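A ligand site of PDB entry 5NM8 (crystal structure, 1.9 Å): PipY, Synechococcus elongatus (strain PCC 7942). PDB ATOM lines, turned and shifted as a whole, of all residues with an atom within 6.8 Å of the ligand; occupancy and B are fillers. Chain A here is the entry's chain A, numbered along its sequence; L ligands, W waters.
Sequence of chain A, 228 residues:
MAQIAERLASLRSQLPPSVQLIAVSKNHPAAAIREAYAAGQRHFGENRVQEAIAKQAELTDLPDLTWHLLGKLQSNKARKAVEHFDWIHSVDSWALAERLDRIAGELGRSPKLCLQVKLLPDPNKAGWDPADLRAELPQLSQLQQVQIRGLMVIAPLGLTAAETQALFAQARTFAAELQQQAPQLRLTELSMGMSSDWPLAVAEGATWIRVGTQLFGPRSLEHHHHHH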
ATOM      1  N   VAL A  24      17.526   7.439  -0.230  1.00  0.00           N
ATOM      2  CA  VAL A  24      17.456   6.466   0.841  1.00  0.00           C
ATOM      3  C   VAL A  24      15.995   6.040   0.936  1.00  0.00           C
ATOM      4  O   VAL A  24      15.156   6.781   1.463  1.00  0.00           O
ATOM      5  CB  VAL A  24      17.980   7.076   2.167  1.00  0.00           C
ATOM      6  CG1 VAL A  24      17.743   6.099   3.322  1.00  0.00           C
ATOM      7  CG2 VAL A  24      19.447   7.358   2.044  1.00  0.00           C
ATOM      8  N   LYS A  26      14.684   3.305   2.510  1.00  0.00           N
ATOM      9  CA  LYS A  26      14.270   2.554   3.677  1.00  0.00           C
ATOM     10  C   LYS A  26      12.911   3.103   4.168  1.00  0.00           C
ATOM     11  O   LYS A  26      12.707   4.307   4.143  1.00  0.00           O
ATOM     12  CB  LYS A  26      15.331   2.617   4.792  1.00  0.00           C
ATOM     13  CG  LYS A  26      15.129   3.779   5.759  1.00  0.00           C
ATOM     14  CD  LYS A  26      16.191   3.927   6.844  1.00  0.00           C
ATOM     15  CE  LYS A  26      16.999   5.176   6.581  1.00  0.00           C
ATOM     16  NZ  LYS A  26      17.438   5.785   7.832  1.00  0.00           N
ATOM     17  N   ASN A  27      11.991   2.239   4.560  1.00  0.00           N
ATOM     18  CA  ASN A  27      10.624   2.677   5.046  1.00  0.00           C
ATOM     19  C   ASN A  27       9.717   3.298   3.967  1.00  0.00           C
ATOM     20  O   ASN A  27       8.762   4.001   4.279  1.00  0.00           O
ATOM     21  CB  ASN A  27      10.694   3.652   6.258  1.00  0.00           C
ATOM     22  CG  ASN A  27      11.533   3.119   7.425  1.00  0.00           C
ATOM     23  OD1 ASN A  27      11.471   1.928   7.763  1.00  0.00           O
ATOM     24  ND2 ASN A  27      12.312   3.980   8.030  1.00  0.00           N
ATOM     25  N   ASN A  47      18.695   0.207   4.786  1.00  0.00           N
ATOM     26  CA  ASN A  47      19.406  -0.172   6.024  1.00  0.00           C
ATOM     27  C   ASN A  47      19.289  -1.620   6.412  1.00  0.00           C
ATOM     28  O   ASN A  47      20.045  -2.070   7.254  1.00  0.00           O
ATOM     29  CB  ASN A  47      19.005   0.720   7.192  1.00  0.00           C
ATOM     30  CG  ASN A  47      19.552   2.105   7.059  1.00  0.00           C
ATOM     31  OD1 ASN A  47      19.434   2.700   5.979  1.00  0.00           O
ATOM     32  ND2 ASN A  47      20.104   2.646   8.116  1.00  0.00           N
ATOM     33  N   LEU A  70      23.270   0.806   4.084  1.00  0.00           N
ATOM     34  CA  LEU A  70      23.589   1.902   5.013  1.00  0.00           C
ATOM     35  C   LEU A  70      23.486   1.523   6.466  1.00  0.00           C
ATOM     36  O   LEU A  70      23.973   2.272   7.316  1.00  0.00           O
ATOM     37  CB  LEU A  70      22.688   3.090   4.741  1.00  0.00           C
ATOM     38  CG  LEU A  70      22.669   3.553   3.252  1.00  0.00           C
ATOM     39  CD1 LEU A  70      21.725   4.652   3.085  1.00  0.00           C
ATOM     40  CD2 LEU A  70      24.064   3.933   2.724  1.00  0.00           C
ATOM     41  N   GLY A  71      22.934   0.367   6.791  1.00  0.00           N
ATOM     42  CA  GLY A  71      22.766  -0.032   8.171  1.00  0.00           C
ATOM     43  C   GLY A  71      23.762  -1.057   8.668  1.00  0.00           C
ATOM     44  O   GLY A  71      24.530  -1.673   7.905  1.00  0.00           O
ATOM     45  N   GLN A 116      32.881   3.000   8.229  1.00  0.00           N
ATOM     46  CA  GLN A 116      32.033   3.879   9.055  1.00  0.00           C
ATOM     47  C   GLN A 116      32.807   4.229  10.306  1.00  0.00           C
ATOM     48  O   GLN A 116      33.112   3.344  11.053  1.00  0.00           O
ATOM     49  CB  GLN A 116      30.737   3.183   9.405  1.00  0.00           C
ATOM     50  CG  GLN A 116      29.766   4.004  10.231  1.00  0.00           C
ATOM     51  CD  GLN A 116      28.500   3.250  10.580  1.00  0.00           C
ATOM     52  OE1 GLN A 116      28.003   2.514   9.786  1.00  0.00           O
ATOM     53  NE2 GLN A 116      27.981   3.447  11.773  1.00  0.00           N
ATOM     54  N   LYS A 125      24.814   4.790  17.203  1.00  0.00           N
ATOM     55  CA  LYS A 125      25.468   4.193  16.013  1.00  0.00           C
ATOM     56  C   LYS A 125      26.794   3.562  16.396  1.00  0.00           C
ATOM     57  O   LYS A 125      27.467   4.030  17.288  1.00  0.00           O
ATOM     58  CB  LYS A 125      25.734   5.223  14.911  1.00  0.00           C
ATOM     59  CG  LYS A 125      24.489   5.815  14.287  1.00  0.00           C
ATOM     60  CD  LYS A 125      23.755   4.803  13.429  1.00  0.00           C
ATOM     61  CE  LYS A 125      22.538   5.436  12.781  1.00  0.00           C
ATOM     62  NZ  LYS A 125      21.291   5.270  13.587  1.00  0.00           N
ATOM     63  N   MET A 152      32.500   6.721   5.856  1.00  0.00           N
ATOM     64  CA  MET A 152      31.137   7.118   6.141  1.00  0.00           C
ATOM     65  C   MET A 152      31.073   7.711   7.518  1.00  0.00           C
ATOM     66  O   MET A 152      31.520   7.081   8.482  1.00  0.00           O
ATOM     67  CB  MET A 152      30.131   5.962   6.073  1.00  0.00           C
ATOM     68  CG  MET A 152      28.704   6.373   6.417  1.00  0.00           C
ATOM     69  SD  MET A 152      27.636   4.945   6.741  1.00  0.00           S
ATOM     70  CE  MET A 152      26.240   5.683   6.002  1.00  0.00           C
ATOM     71  N   ILE A 154      28.244   9.637  10.221  1.00  0.00           N
ATOM     72  CA  ILE A 154      26.857   9.941  10.542  1.00  0.00           C
ATOM     73  C   ILE A 154      26.907  10.830  11.811  1.00  0.00           C
ATOM     74  O   ILE A 154      27.579  10.476  12.818  1.00  0.00           O
ATOM     75  CB  ILE A 154      26.062   8.674  10.886  1.00  0.00           C
ATOM     76  CG1 ILE A 154      26.147   7.615   9.775  1.00  0.00           C
ATOM     77  CG2 ILE A 154      24.621   9.009  11.215  1.00  0.00           C
ATOM     78  CD1 ILE A 154      25.791   6.202  10.233  1.00  0.00           C
ATOM     79  N   GLY A 193      26.199  13.300   5.068  1.00  0.00           N
ATOM     80  CA  GLY A 193      25.125  14.234   4.818  1.00  0.00           C
ATOM     81  C   GLY A 193      23.822  13.497   4.560  1.00  0.00           C
ATOM     82  O   GLY A 193      23.726  12.659   3.660  1.00  0.00           O
ATOM     83  N   MET A 194      22.810  13.865   5.298  1.00  0.00           N
ATOM     84  CA  MET A 194      21.484  13.332   5.190  1.00  0.00           C
ATOM     85  C   MET A 194      20.509  14.489   5.038  1.00  0.00           C
ATOM     86  O   MET A 194      20.958  15.620   4.789  1.00  0.00           O
ATOM     87  CB  MET A 194      21.195  12.455   6.397  1.00  0.00           C
ATOM     88  CG  MET A 194      22.207  11.319   6.521  1.00  0.00           C
ATOM     89  SD  MET A 194      22.399  10.565   8.174  1.00  0.00           S
ATOM     90  CE  MET A 194      20.717  10.517   8.741  1.00  0.00           C
ATOM     91  N   SER A 195      19.211  14.243   5.180  1.00  0.00           N
ATOM     92  CA  SER A 195      18.210  15.269   4.833  1.00  0.00           C
ATOM     93  C   SER A 195      18.449  16.594   5.501  1.00  0.00           C
ATOM     94  O   SER A 195      18.364  17.627   4.865  1.00  0.00           O
ATOM     95  CB  SER A 195      16.782  14.824   5.159  1.00  0.00           C
ATOM     96  OG  SER A 195      16.323  13.897   4.193  1.00  0.00           O
ATOM     97  N   SER A 196      18.774  16.572   6.778  1.00  0.00           N
ATOM     98  CA  SER A 196      18.909  17.821   7.491  1.00  0.00           C
ATOM     99  C   SER A 196      20.265  18.517   7.294  1.00  0.00           C
ATOM    100  O   SER A 196      20.389  19.731   7.455  1.00  0.00           O
ATOM    101  CB  SER A 196      18.607  17.574   8.979  1.00  0.00           C
ATOM    102  OG  SER A 196      19.697  16.876   9.605  1.00  0.00           O
ATOM    103  N   ARG A 210      23.193  11.145   1.360  1.00  0.00           N
ATOM    104  CA  ARG A 210      22.241  10.051   1.615  1.00  0.00           C
ATOM    105  C   ARG A 210      20.965  10.657   2.090  1.00  0.00           C
ATOM    106  O   ARG A 210      20.810  10.947   3.271  1.00  0.00           O
ATOM    107  CB  ARG A 210      22.808   9.050   2.671  1.00  0.00           C
ATOM    108  CG  ARG A 210      24.130   8.385   2.260  1.00  0.00           C
ATOM    109  CD  ARG A 210      24.700   7.420   3.341  1.00  0.00           C
ATOM    110  NE  ARG A 210      24.435   7.939   4.679  1.00  0.00           N
ATOM    111  CZ  ARG A 210      25.254   8.661   5.434  1.00  0.00           C
ATOM    112  NH1 ARG A 210      26.499   8.880   5.099  1.00  0.00           N
ATOM    113  NH2 ARG A 210      24.821   9.077   6.589  1.00  0.00           N
ATOM    114  N   VAL A 211      20.037  10.895   1.160  1.00  0.00           N
ATOM    115  CA  VAL A 211      18.864  11.650   1.499  1.00  0.00           C
ATOM    116  C   VAL A 211      17.614  10.802   1.402  1.00  0.00           C
ATOM    117  O   VAL A 211      17.313  10.209   0.356  1.00  0.00           O
ATOM    118  CB  VAL A 211      18.751  12.891   0.585  1.00  0.00           C
ATOM    119  CG1 VAL A 211      17.511  13.638   0.857  1.00  0.00           C
ATOM    120  CG2 VAL A 211      19.927  13.855   0.809  1.00  0.00           C
ATOM    121  N   GLY A 212      16.850  10.767   2.484  1.00  0.00           N
ATOM    122  CA  GLY A 212      15.594   9.988   2.495  1.00  0.00           C
ATOM    123  C   GLY A 212      14.352  10.864   2.569  1.00  0.00           C
ATOM    124  O   GLY A 212      13.634  11.065   1.561  1.00  0.00           O
ATOM    125  N   THR A 213      14.065  11.339   3.768  1.00  0.00           N
ATOM    126  CA  THR A 213      12.870  12.121   4.053  1.00  0.00           C
ATOM    127  C   THR A 213      12.636  13.321   3.137  1.00  0.00           C
ATOM    128  O   THR A 213      11.543  13.500   2.589  1.00  0.00           O
ATOM    129  CB  THR A 213      12.922  12.569   5.507  1.00  0.00           C
ATOM    130  OG1 THR A 213      13.100  11.398   6.331  1.00  0.00           O
ATOM    131  CG2 THR A 213      11.657  13.306   5.892  1.00  0.00           C
ATOM    132  N   GLN A 214      13.665  14.117   2.893  1.00  0.00           N
ATOM    133  CA  GLN A 214      13.453  15.267   1.976  1.00  0.00           C
ATOM    134  C   GLN A 214      12.973  14.855   0.569  1.00  0.00           C
ATOM    135  O   GLN A 214      12.312  15.653  -0.088  1.00  0.00           O
ATOM    136  CB  GLN A 214      14.697  16.121   1.865  1.00  0.00           C
ATOM    137  CG  GLN A 214      14.554  17.333   0.967  1.00  0.00           C
ATOM    138  CD  GLN A 214      15.872  18.064   0.779  1.00  0.00           C
ATOM    139  OE1 GLN A 214      16.627  18.292   1.734  1.00  0.00           O
ATOM    140  NE2 GLN A 214      16.142  18.461  -0.461  1.00  0.00           N
ATOM    141  N   GLY A 217       9.508  12.103   1.567  1.00  0.00           N
ATOM    142  CA  GLY A 217       8.624  12.484   2.652  1.00  0.00           C
ATOM    143  C   GLY A 217       8.675  11.457   3.777  1.00  0.00           C
ATOM    144  O   GLY A 217       9.512  10.539   3.757  1.00  0.00           O
HETATM  145  N1  LIG L   1      21.814   7.442   5.989  1.00  0.00           N
HETATM  146  C1  LIG L   1      21.682   6.523   6.980  1.00  0.00           C
HETATM  147  C2  LIG L   1      22.855   5.700   7.452  1.00  0.00           C
HETATM  148  C3  LIG L   1      20.375   6.328   7.615  1.00  0.00           C
HETATM  149  O1  LIG L   1      20.221   5.431   8.618  1.00  0.00           O
HETATM  150  C4  LIG L   1      19.229   7.135   7.139  1.00  0.00           C
HETATM  151  C5  LIG L   1      17.894   6.967   7.771  1.00  0.00           C
HETATM  152  C6  LIG L   1      19.495   8.107   6.043  1.00  0.00           C
HETATM  153  C7  LIG L   1      20.785   8.187   5.531  1.00  0.00           C
HETATM  154  C8  LIG L   1      18.398   8.992   5.526  1.00  0.00           C
HETATM  155  O2  LIG L   1      18.025   9.911   6.579  1.00  0.00           O
HETATM  156  P1  LIG L   1      17.044  11.153   6.255  1.00  0.00           P
HETATM  157  O3  LIG L   1      17.660  11.788   5.023  1.00  0.00           O
HETATM  158  O4  LIG L   1      17.120  11.978   7.503  1.00  0.00           O
HETATM  159  O5  LIG L   1      15.651  10.560   6.021  1.00  0.00           O
HETATM  160  O   HOH W   1      14.859   8.029   6.044  1.00  0.00           O
HETATM  161  O   HOH W   2      18.539  14.033   8.282  1.00  0.00           O
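C5 of the ligand is covalently linked to NZ of Lys 26, at 1.3 Å. N of Ser 195 sits at hydrogen-bond distance from O3 of the ligand, at 2.9 Å. OG of Ser 195 sits at hydrogen-bond distance from O3 of the ligand (2.6 Å). N of Thr 213 sits at hydrogen-bond distance from O5 of the ligand. The side-chain hydroxyl (OG1) of Thr 213 is in hydrogen-bond range of an oxygen (O5) of the ligand (2.7 Å). The side-chain amide nitrogen (ND2) of Asn 47 sits at hydrogen-bond distance from an oxygen (O1) of the ligand, 2.8 Å away. N of Gly 212 lies within hydrogen-bond range of O3 of the ligand (2.9 Å). The guanidinium group of Arg 210 is in hydrogen-bond range of a nitrogen (N1) of the ligand, at 3.0 Å.
The side-chain hydroxyl of Ser 195 lies within hydrogen-bond range of the backbone NH of Thr 213 (3.4 Å). N of Gln 214 lies within hydrogen-bond range of OG of Ser 195 (3.0 Å). NH2 of Arg 210 is in hydrogen-bond range of SD of Met 194 (3.3 Å). The backbone carbonyl oxygen (O) of Gly 193 lies within hydrogen-bond range of the backbone NH (N) of Arg 210 (2.8 Å). The backbone NH (N) of Val 24 lies within hydrogen-bond range of the backbone carbonyl oxygen (O) of Val 211 (2.8 Å).
Residues that only touch the ligand: Val 24, Leu 70, Met 152, Met 194 and Val 211. Of the 20 residues printed, 11 come within 4 Å of the ligand.
Water W2 lies within hydrogen-bond range of an oxygen (O4) of the ligand (2.6 Å), the backbone NH of Ser 196 (3.0 Å) and the backbone NH of Ser 195 (3.2 Å).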
